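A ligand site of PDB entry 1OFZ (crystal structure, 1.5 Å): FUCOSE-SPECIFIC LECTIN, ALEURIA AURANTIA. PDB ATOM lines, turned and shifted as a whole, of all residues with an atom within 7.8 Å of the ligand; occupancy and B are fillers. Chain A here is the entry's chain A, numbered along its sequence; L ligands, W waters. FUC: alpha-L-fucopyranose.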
ATOM      1  N   ILE A 173       6.721  -5.949  16.418  1.00  0.00           N
ATOM      2  CA  ILE A 173       5.276  -5.841  16.659  1.00  0.00           C
ATOM      3  C   ILE A 173       4.820  -6.676  17.839  1.00  0.00           C
ATOM      4  O   ILE A 173       3.683  -6.524  18.303  1.00  0.00           O
ATOM      5  CB  ILE A 173       4.466  -6.207  15.371  1.00  0.00           C
ATOM      6  CG1 ILE A 173       4.595  -7.690  15.000  1.00  0.00           C
ATOM      7  CG2 ILE A 173       4.890  -5.345  14.208  1.00  0.00           C
ATOM      8  CD1 ILE A 173       3.653  -8.134  13.866  1.00  0.00           C
ATOM      9  N   ARG A 177       8.788 -10.795  17.303  1.00  0.00           N
ATOM     10  CA  ARG A 177       7.961 -10.800  16.103  1.00  0.00           C
ATOM     11  C   ARG A 177       8.261  -9.510  15.348  1.00  0.00           C
ATOM     12  O   ARG A 177       7.975  -8.420  15.824  1.00  0.00           O
ATOM     13  CB  ARG A 177       6.480 -10.841  16.513  1.00  0.00           C
ATOM     14  CG  ARG A 177       5.540 -11.144  15.405  1.00  0.00           C
ATOM     15  CD  ARG A 177       4.108 -11.443  15.950  1.00  0.00           C
ATOM     16  NE  ARG A 177       3.184 -11.772  14.884  1.00  0.00           N
ATOM     17  CZ  ARG A 177       1.916 -11.400  14.823  1.00  0.00           C
ATOM     18  NH1 ARG A 177       1.376 -10.662  15.794  1.00  0.00           N
ATOM     19  NH2 ARG A 177       1.201 -11.799  13.796  1.00  0.00           N
ATOM     20  N   LEU A 178       8.885  -9.655  14.183  1.00  0.00           N
ATOM     21  CA  LEU A 178       9.534  -8.547  13.494  1.00  0.00           C
ATOM     22  C   LEU A 178       8.889  -8.278  12.167  1.00  0.00           C
ATOM     23  O   LEU A 178       8.538  -9.195  11.452  1.00  0.00           O
ATOM     24  CB  LEU A 178      11.016  -8.836  13.294  1.00  0.00           C
ATOM     25  CG  LEU A 178      11.760  -9.411  14.475  1.00  0.00           C
ATOM     26  CD1 LEU A 178      13.255  -9.652  14.125  1.00  0.00           C
ATOM     27  CD2 LEU A 178      11.627  -8.551  15.715  1.00  0.00           C
ATOM     28  N   ARG A 179       8.809  -7.011  11.772  1.00  0.00           N
ATOM     29  CA  ARG A 179       8.366  -6.593  10.461  1.00  0.00           C
ATOM     30  C   ARG A 179       9.304  -5.577   9.891  1.00  0.00           C
ATOM     31  O   ARG A 179       9.624  -4.585  10.544  1.00  0.00           O
ATOM     32  CB  ARG A 179       6.934  -6.054  10.503  1.00  0.00           C
ATOM     33  CG  ARG A 179       5.882  -7.037  10.941  1.00  0.00           C
ATOM     34  CD  ARG A 179       5.714  -8.185   9.944  1.00  0.00           C
ATOM     35  NE  ARG A 179       4.664  -9.133  10.318  1.00  0.00           N
ATOM     36  CZ  ARG A 179       4.813 -10.164  11.116  1.00  0.00           C
ATOM     37  NH1 ARG A 179       5.958 -10.441  11.697  1.00  0.00           N
ATOM     38  NH2 ARG A 179       3.773 -10.992  11.351  1.00  0.00           N
ATOM     39  N   ILE A 180       9.782  -5.839   8.690  1.00  0.00           N
ATOM     40  CA  ILE A 180      10.730  -5.008   7.979  1.00  0.00           C
ATOM     41  C   ILE A 180      10.095  -4.539   6.692  1.00  0.00           C
ATOM     42  O   ILE A 180       9.599  -5.347   5.895  1.00  0.00           O
ATOM     43  CB  ILE A 180      12.044  -5.792   7.660  1.00  0.00           C
ATOM     44  CG1 ILE A 180      12.609  -6.521   8.858  1.00  0.00           C
ATOM     45  CG2 ILE A 180      13.066  -4.891   7.034  1.00  0.00           C
ATOM     46  CD1 ILE A 180      12.923  -5.652  10.039  1.00  0.00           C
ATOM     47  N   TYR A 181      10.175  -3.232   6.438  1.00  0.00           N
ATOM     48  CA  TYR A 181       9.600  -2.616   5.271  1.00  0.00           C
ATOM     49  C   TYR A 181      10.693  -1.982   4.444  1.00  0.00           C
ATOM     50  O   TYR A 181      11.603  -1.375   4.982  1.00  0.00           O
ATOM     51  CB  TYR A 181       8.517  -1.567   5.673  1.00  0.00           C
ATOM     52  CG  TYR A 181       7.445  -2.222   6.491  1.00  0.00           C
ATOM     53  CD1 TYR A 181       6.377  -2.826   5.881  1.00  0.00           C
ATOM     54  CD2 TYR A 181       7.550  -2.308   7.881  1.00  0.00           C
ATOM     55  CE1 TYR A 181       5.461  -3.521   6.608  1.00  0.00           C
ATOM     56  CE2 TYR A 181       6.625  -3.003   8.623  1.00  0.00           C
ATOM     57  CZ  TYR A 181       5.576  -3.634   7.970  1.00  0.00           C
ATOM     58  OH  TYR A 181       4.631  -4.338   8.707  1.00  0.00           O
ATOM     59  N   GLU A 191       7.205  -6.097   2.490  1.00  0.00           N
ATOM     60  CA  GLU A 191       7.275  -6.412   3.873  1.00  0.00           C
ATOM     61  C   GLU A 191       7.897  -7.793   4.047  1.00  0.00           C
ATOM     62  O   GLU A 191       7.518  -8.747   3.327  1.00  0.00           O
ATOM     63  CB  GLU A 191       5.856  -6.420   4.447  1.00  0.00           C
ATOM     64  CG  GLU A 191       5.707  -6.856   5.886  1.00  0.00           C
ATOM     65  CD  GLU A 191       4.266  -7.037   6.295  1.00  0.00           C
ATOM     66  OE1 GLU A 191       3.526  -7.733   5.559  1.00  0.00           O
ATOM     67  OE2 GLU A 191       3.850  -6.446   7.315  1.00  0.00           O
ATOM     68  N   HIS A 192       8.848  -7.910   4.954  1.00  0.00           N
ATOM     69  CA  HIS A 192       9.414  -9.185   5.380  1.00  0.00           C
ATOM     70  C   HIS A 192       9.131  -9.389   6.841  1.00  0.00           C
ATOM     71  O   HIS A 192       9.177  -8.457   7.646  1.00  0.00           O
ATOM     72  CB  HIS A 192      10.896  -9.226   5.142  1.00  0.00           C
ATOM     73  CG  HIS A 192      11.300 -10.404   4.352  1.00  0.00           C
ATOM     74  ND1 HIS A 192      11.079 -10.474   3.009  1.00  0.00           N
ATOM     75  CD2 HIS A 192      11.845 -11.582   4.721  1.00  0.00           C
ATOM     76  CE1 HIS A 192      11.513 -11.640   2.564  1.00  0.00           C
ATOM     77  NE2 HIS A 192      11.960 -12.336   3.587  1.00  0.00           N
ATOM     78  N   CYS A 193       8.825 -10.633   7.205  1.00  0.00           N
ATOM     79  CA  CYS A 193       8.254 -10.979   8.487  1.00  0.00           C
ATOM     80  C   CYS A 193       9.004 -12.105   9.172  1.00  0.00           C
ATOM     81  O   CYS A 193       9.415 -13.068   8.506  1.00  0.00           O
ATOM     82  CB  CYS A 193       6.834 -11.469   8.310  1.00  0.00           C
ATOM     83  SG  CYS A 193       5.752 -10.440   7.300  1.00  0.00           S
ATOM     84  N   ASP A 195       8.069 -14.419  12.608  1.00  0.00           N
ATOM     85  CA  ASP A 195       7.190 -14.696  13.752  1.00  0.00           C
ATOM     86  C   ASP A 195       7.786 -15.666  14.766  1.00  0.00           C
ATOM     87  O   ASP A 195       7.557 -15.528  15.962  1.00  0.00           O
ATOM     88  CB  ASP A 195       5.863 -15.324  13.270  1.00  0.00           C
ATOM     89  CG  ASP A 195       4.951 -14.344  12.566  1.00  0.00           C
ATOM     90  OD1 ASP A 195       4.946 -13.122  12.889  1.00  0.00           O
ATOM     91  OD2 ASP A 195       4.158 -14.741  11.682  1.00  0.00           O
ATOM     92  N   TYR A 200       9.682 -14.660   6.137  1.00  0.00           N
ATOM     93  CA  TYR A 200       8.805 -14.880   5.001  1.00  0.00           C
ATOM     94  C   TYR A 200       8.269 -13.568   4.494  1.00  0.00           C
ATOM     95  O   TYR A 200       8.269 -12.533   5.195  1.00  0.00           O
ATOM     96  CB  TYR A 200       7.666 -15.805   5.410  1.00  0.00           C
ATOM     97  CG  TYR A 200       6.700 -15.260   6.428  1.00  0.00           C
ATOM     98  CD1 TYR A 200       5.571 -14.541   6.037  1.00  0.00           C
ATOM     99  CD2 TYR A 200       6.891 -15.453   7.798  1.00  0.00           C
ATOM    100  CE1 TYR A 200       4.681 -14.048   6.964  1.00  0.00           C
ATOM    101  CE2 TYR A 200       6.012 -14.952   8.731  1.00  0.00           C
ATOM    102  CZ  TYR A 200       4.882 -14.269   8.305  1.00  0.00           C
ATOM    103  OH  TYR A 200       4.016 -13.795   9.252  1.00  0.00           O
ATOM    104  N   VAL A 201       7.794 -13.598   3.272  1.00  0.00           N
ATOM    105  CA  VAL A 201       7.265 -12.415   2.624  1.00  0.00           C
ATOM    106  C   VAL A 201       5.860 -12.096   3.150  1.00  0.00           C
ATOM    107  O   VAL A 201       4.936 -12.918   3.092  1.00  0.00           O
ATOM    108  CB  VAL A 201       7.191 -12.640   1.108  1.00  0.00           C
ATOM    109  CG1 VAL A 201       6.529 -11.458   0.436  1.00  0.00           C
ATOM    110  CG2 VAL A 201       8.529 -12.893   0.558  1.00  0.00           C
ATOM    111  N   GLY A 202       5.682 -10.891   3.679  1.00  0.00           N
ATOM    112  CA  GLY A 202       4.402 -10.485   4.200  1.00  0.00           C
ATOM    113  C   GLY A 202       3.399 -10.111   3.130  1.00  0.00           C
ATOM    114  O   GLY A 202       3.758  -9.927   1.947  1.00  0.00           O
ATOM    115  N   GLY A 203       2.138  -9.996   3.533  1.00  0.00           N
ATOM    116  CA  GLY A 203       1.072  -9.645   2.646  1.00  0.00           C
ATOM    117  C   GLY A 203       1.043  -8.206   2.158  1.00  0.00           C
ATOM    118  O   GLY A 203       0.352  -7.859   1.182  1.00  0.00           O
ATOM    119  N   PHE A 204       1.750  -7.342   2.879  1.00  0.00           N
ATOM    120  CA  PHE A 204       1.667  -5.919   2.581  1.00  0.00           C
ATOM    121  C   PHE A 204       2.461  -5.507   1.371  1.00  0.00           C
ATOM    122  O   PHE A 204       3.594  -5.919   1.232  1.00  0.00           O
ATOM    123  CB  PHE A 204       2.174  -5.072   3.767  1.00  0.00           C
ATOM    124  CG  PHE A 204       2.209  -3.605   3.464  1.00  0.00           C
ATOM    125  CD1 PHE A 204       1.022  -2.894   3.327  1.00  0.00           C
ATOM    126  CD2 PHE A 204       3.409  -2.950   3.203  1.00  0.00           C
ATOM    127  CE1 PHE A 204       1.044  -1.578   2.993  1.00  0.00           C
ATOM    128  CE2 PHE A 204       3.409  -1.628   2.849  1.00  0.00           C
ATOM    129  CZ  PHE A 204       2.249  -0.944   2.767  1.00  0.00           C
ATOM    130  N   SER A 205       1.850  -4.728   0.496  1.00  0.00           N
ATOM    131  CA  SER A 205       2.597  -4.020  -0.544  1.00  0.00           C
ATOM    132  C   SER A 205       1.842  -2.779  -0.974  1.00  0.00           C
ATOM    133  O   SER A 205       0.618  -2.714  -0.879  1.00  0.00           O
ATOM    134  CB  SER A 205       2.918  -4.931  -1.749  1.00  0.00           C
ATOM    135  OG  SER A 205       1.736  -5.197  -2.490  1.00  0.00           O
ATOM    136  N   THR A 222      -3.015  -5.729  19.313  1.00  0.00           N
ATOM    137  CA  THR A 222      -3.773  -6.140  18.127  1.00  0.00           C
ATOM    138  C   THR A 222      -2.969  -6.973  17.107  1.00  0.00           C
ATOM    139  O   THR A 222      -3.493  -7.992  16.627  1.00  0.00           O
ATOM    140  CB  THR A 222      -4.462  -4.911  17.521  1.00  0.00           C
ATOM    141  OG1 THR A 222      -5.475  -4.398  18.430  1.00  0.00           O
ATOM    142  CG2 THR A 222      -5.186  -5.264  16.190  1.00  0.00           C
ATOM    143  N   PRO A 223      -1.739  -6.594  16.727  1.00  0.00           N
ATOM    144  CA  PRO A 223      -1.106  -5.314  17.037  1.00  0.00           C
ATOM    145  C   PRO A 223      -1.409  -4.289  15.961  1.00  0.00           C
ATOM    146  O   PRO A 223      -2.049  -4.584  14.955  1.00  0.00           O
ATOM    147  CB  PRO A 223       0.384  -5.673  16.994  1.00  0.00           C
ATOM    148  CG  PRO A 223       0.426  -6.651  15.891  1.00  0.00           C
ATOM    149  CD  PRO A 223      -0.872  -7.414  15.864  1.00  0.00           C
ATOM    150  N   ASN A 224      -0.912  -3.069  16.162  1.00  0.00           N
ATOM    151  CA  ASN A 224      -1.106  -1.964  15.246  1.00  0.00           C
ATOM    152  C   ASN A 224       0.236  -1.622  14.630  1.00  0.00           C
ATOM    153  O   ASN A 224       1.228  -1.583  15.319  1.00  0.00           O
ATOM    154  CB  ASN A 224      -1.660  -0.741  15.977  1.00  0.00           C
ATOM    155  CG  ASN A 224      -2.888  -1.088  16.754  1.00  0.00           C
ATOM    156  OD1 ASN A 224      -3.989  -1.113  16.209  1.00  0.00           O
ATOM    157  ND2 ASN A 224      -2.696  -1.360  18.062  1.00  0.00           N
ATOM    158  N   ILE A 225       0.254  -1.485  13.314  1.00  0.00           N
ATOM    159  CA  ILE A 225       1.465  -1.146  12.574  1.00  0.00           C
ATOM    160  C   ILE A 225       1.151   0.072  11.759  1.00  0.00           C
ATOM    161  O   ILE A 225       0.036   0.209  11.177  1.00  0.00           O
ATOM    162  CB  ILE A 225       1.924  -2.286  11.616  1.00  0.00           C
ATOM    163  CG1 ILE A 225       1.865  -3.644  12.309  1.00  0.00           C
ATOM    164  CG2 ILE A 225       3.361  -2.000  11.128  1.00  0.00           C
ATOM    165  CD1 ILE A 225       2.160  -4.809  11.422  1.00  0.00           C
ATOM    166  N   TYR A 241      -2.165  -0.906   9.734  1.00  0.00           N
ATOM    167  CA  TYR A 241      -2.613  -2.260   9.999  1.00  0.00           C
ATOM    168  C   TYR A 241      -3.215  -2.296  11.392  1.00  0.00           C
ATOM    169  O   TYR A 241      -2.598  -1.875  12.355  1.00  0.00           O
ATOM    170  CB  TYR A 241      -1.422  -3.227   9.984  1.00  0.00           C
ATOM    171  CG  TYR A 241      -1.785  -4.667  10.235  1.00  0.00           C
ATOM    172  CD1 TYR A 241      -2.149  -5.518   9.179  1.00  0.00           C
ATOM    173  CD2 TYR A 241      -1.721  -5.190  11.501  1.00  0.00           C
ATOM    174  CE1 TYR A 241      -2.441  -6.868   9.395  1.00  0.00           C
ATOM    175  CE2 TYR A 241      -2.039  -6.549  11.755  1.00  0.00           C
ATOM    176  CZ  TYR A 241      -2.367  -7.368  10.681  1.00  0.00           C
ATOM    177  OH  TYR A 241      -2.687  -8.700  10.935  1.00  0.00           O
ATOM    178  N   GLY A 243      -5.131  -5.442  12.000  1.00  0.00           N
ATOM    179  CA  GLY A 243      -5.655  -6.763  11.760  1.00  0.00           C
ATOM    180  C   GLY A 243      -5.795  -7.021  10.278  1.00  0.00           C
ATOM    181  O   GLY A 243      -5.719  -8.162   9.785  1.00  0.00           O
ATOM    182  N   SER A 244      -5.992  -5.921   9.568  1.00  0.00           N
ATOM    183  CA  SER A 244      -5.929  -5.874   8.114  1.00  0.00           C
ATOM    184  C   SER A 244      -5.248  -4.576   7.703  1.00  0.00           C
ATOM    185  O   SER A 244      -5.184  -3.622   8.499  1.00  0.00           O
ATOM    186  CB  SER A 244      -7.331  -5.991   7.511  1.00  0.00           C
ATOM    187  OG  SER A 244      -8.108  -4.844   7.808  1.00  0.00           O
ATOM    188  N   TRP A 245      -4.776  -4.499   6.470  1.00  0.00           N
ATOM    189  CA  TRP A 245      -4.191  -3.265   5.940  1.00  0.00           C
ATOM    190  C   TRP A 245      -5.239  -2.387   5.327  1.00  0.00           C
ATOM    191  O   TRP A 245      -6.170  -2.861   4.654  1.00  0.00           O
ATOM    192  CB  TRP A 245      -3.083  -3.524   4.927  1.00  0.00           C
ATOM    193  CG  TRP A 245      -1.866  -4.101   5.528  1.00  0.00           C
ATOM    194  CD1 TRP A 245      -1.522  -5.417   5.555  1.00  0.00           C
ATOM    195  CD2 TRP A 245      -0.827  -3.406   6.231  1.00  0.00           C
ATOM    196  NE1 TRP A 245      -0.335  -5.590   6.230  1.00  0.00           N
ATOM    197  CE2 TRP A 245       0.112  -4.372   6.663  1.00  0.00           C
ATOM    198  CE3 TRP A 245      -0.580  -2.060   6.537  1.00  0.00           C
ATOM    199  CZ2 TRP A 245       1.275  -4.029   7.368  1.00  0.00           C
ATOM    200  CZ3 TRP A 245       0.604  -1.738   7.234  1.00  0.00           C
ATOM    201  CH2 TRP A 245       1.480  -2.708   7.643  1.00  0.00           C
HETATM  202  C1  FUC L   1       1.362 -11.171   8.550  1.00  0.00           C
HETATM  203  C2  FUC L   1       1.669 -10.261   7.353  1.00  0.00           C
HETATM  204  C3  FUC L   1       0.846  -8.985   7.445  1.00  0.00           C
HETATM  205  C4  FUC L   1       1.059  -8.326   8.815  1.00  0.00           C
HETATM  206  C5  FUC L   1       0.709  -9.311   9.932  1.00  0.00           C
HETATM  207  C6  FUC L   1       0.912  -8.745  11.340  1.00  0.00           C
HETATM  208  O1  FUC L   1       0.034 -11.654   8.407  1.00  0.00           O
HETATM  209  O2  FUC L   1       1.429 -10.942   6.120  1.00  0.00           O
HETATM  210  O3  FUC L   1       1.064  -8.094   6.356  1.00  0.00           O
HETATM  211  O4  FUC L   1       2.437  -7.981   8.970  1.00  0.00           O
HETATM  212  O5  FUC L   1       1.502 -10.476   9.797  1.00  0.00           O
HETATM  213  O   HOH W   1      -1.105  -8.635   4.682  1.00  0.00           O
HETATM  214  O   HOH W   2       1.028 -13.634   6.224  1.00  0.00           O
HETATM  215  O   HOH W   3      -1.404 -11.574   5.668  1.00  0.00           O
HETATM  216  O   HOH W   4      -2.939 -10.257   8.510  1.00  0.00           O
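Water W4 lies within hydrogen-bond range of the side-chain hydroxyl (OH) of Tyr 241 and an oxygen (O1) of the ligand.
An oxygen (O5) of the ligand is in hydrogen-bond range of the guanidinium group of Arg 179, 2.8 Å away. An oxygen (O2) of the ligand sits at hydrogen-bond distance from the backbone NH (N) of Gly 203, 2.8 Å away. NE1 of Trp 245 is in hydrogen-bond range of O3 of the ligand (2.9 Å). An oxygen (O3) of the ligand is in hydrogen-bond range of the side-chain carboxylate (OE1) of Glu 191 (2.6 Å).
Ile 173 touches the ligand (CD1 to C6, 3.8 Å). NH2 of Arg 177 touches C6 of the ligand (3.9 Å). Tyr 200 touches the ligand (OH to C1, 3.8 Å). CA of Gly 202 touches O2 of the ligand (3.6 Å). N of Phe 204 touches O3 of the ligand, 3.6 Å away. Tyr 241 touches the ligand (OH to C5, 3.6 Å). Within 4 Å of the ligand: Ile 173, Arg 177, Arg 179, Glu 191, Tyr 200, Gly 202, Gly 203, Phe 204, Tyr 241 and Trp 245.
OE1 of Glu 191 lies within hydrogen-bond range of N of Gly 203 (3.3 Å). NE of Arg 177 lies within salt-bridge range of OD1 of Asp 195 (3.0 Å). The side-chain hydroxyl (OH) of Tyr 200 sits at hydrogen-bond distance from the side-chain carboxylate (OD2) of Asp 195, 2.6 Å away. The side-chain hydroxyl (OH) of Tyr 181 lies within hydrogen-bond range of the side-chain carboxylate (OE2) of Glu 191 (2.6 Å). The backbone NH of Tyr 241 sits at hydrogen-bond distance from the backbone carbonyl oxygen of Ile 225 (2.9 Å). N of Cys 193 lies within hydrogen-bond range of O of Tyr 200, at 2.8 Å. The side-chain sulfur of Cys 193 lies close to the backbone NH of Gly 202 (3.6 Å). O of Gly 243 is in hydrogen-bond range of OH of Tyr 241 (3.3 Å).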
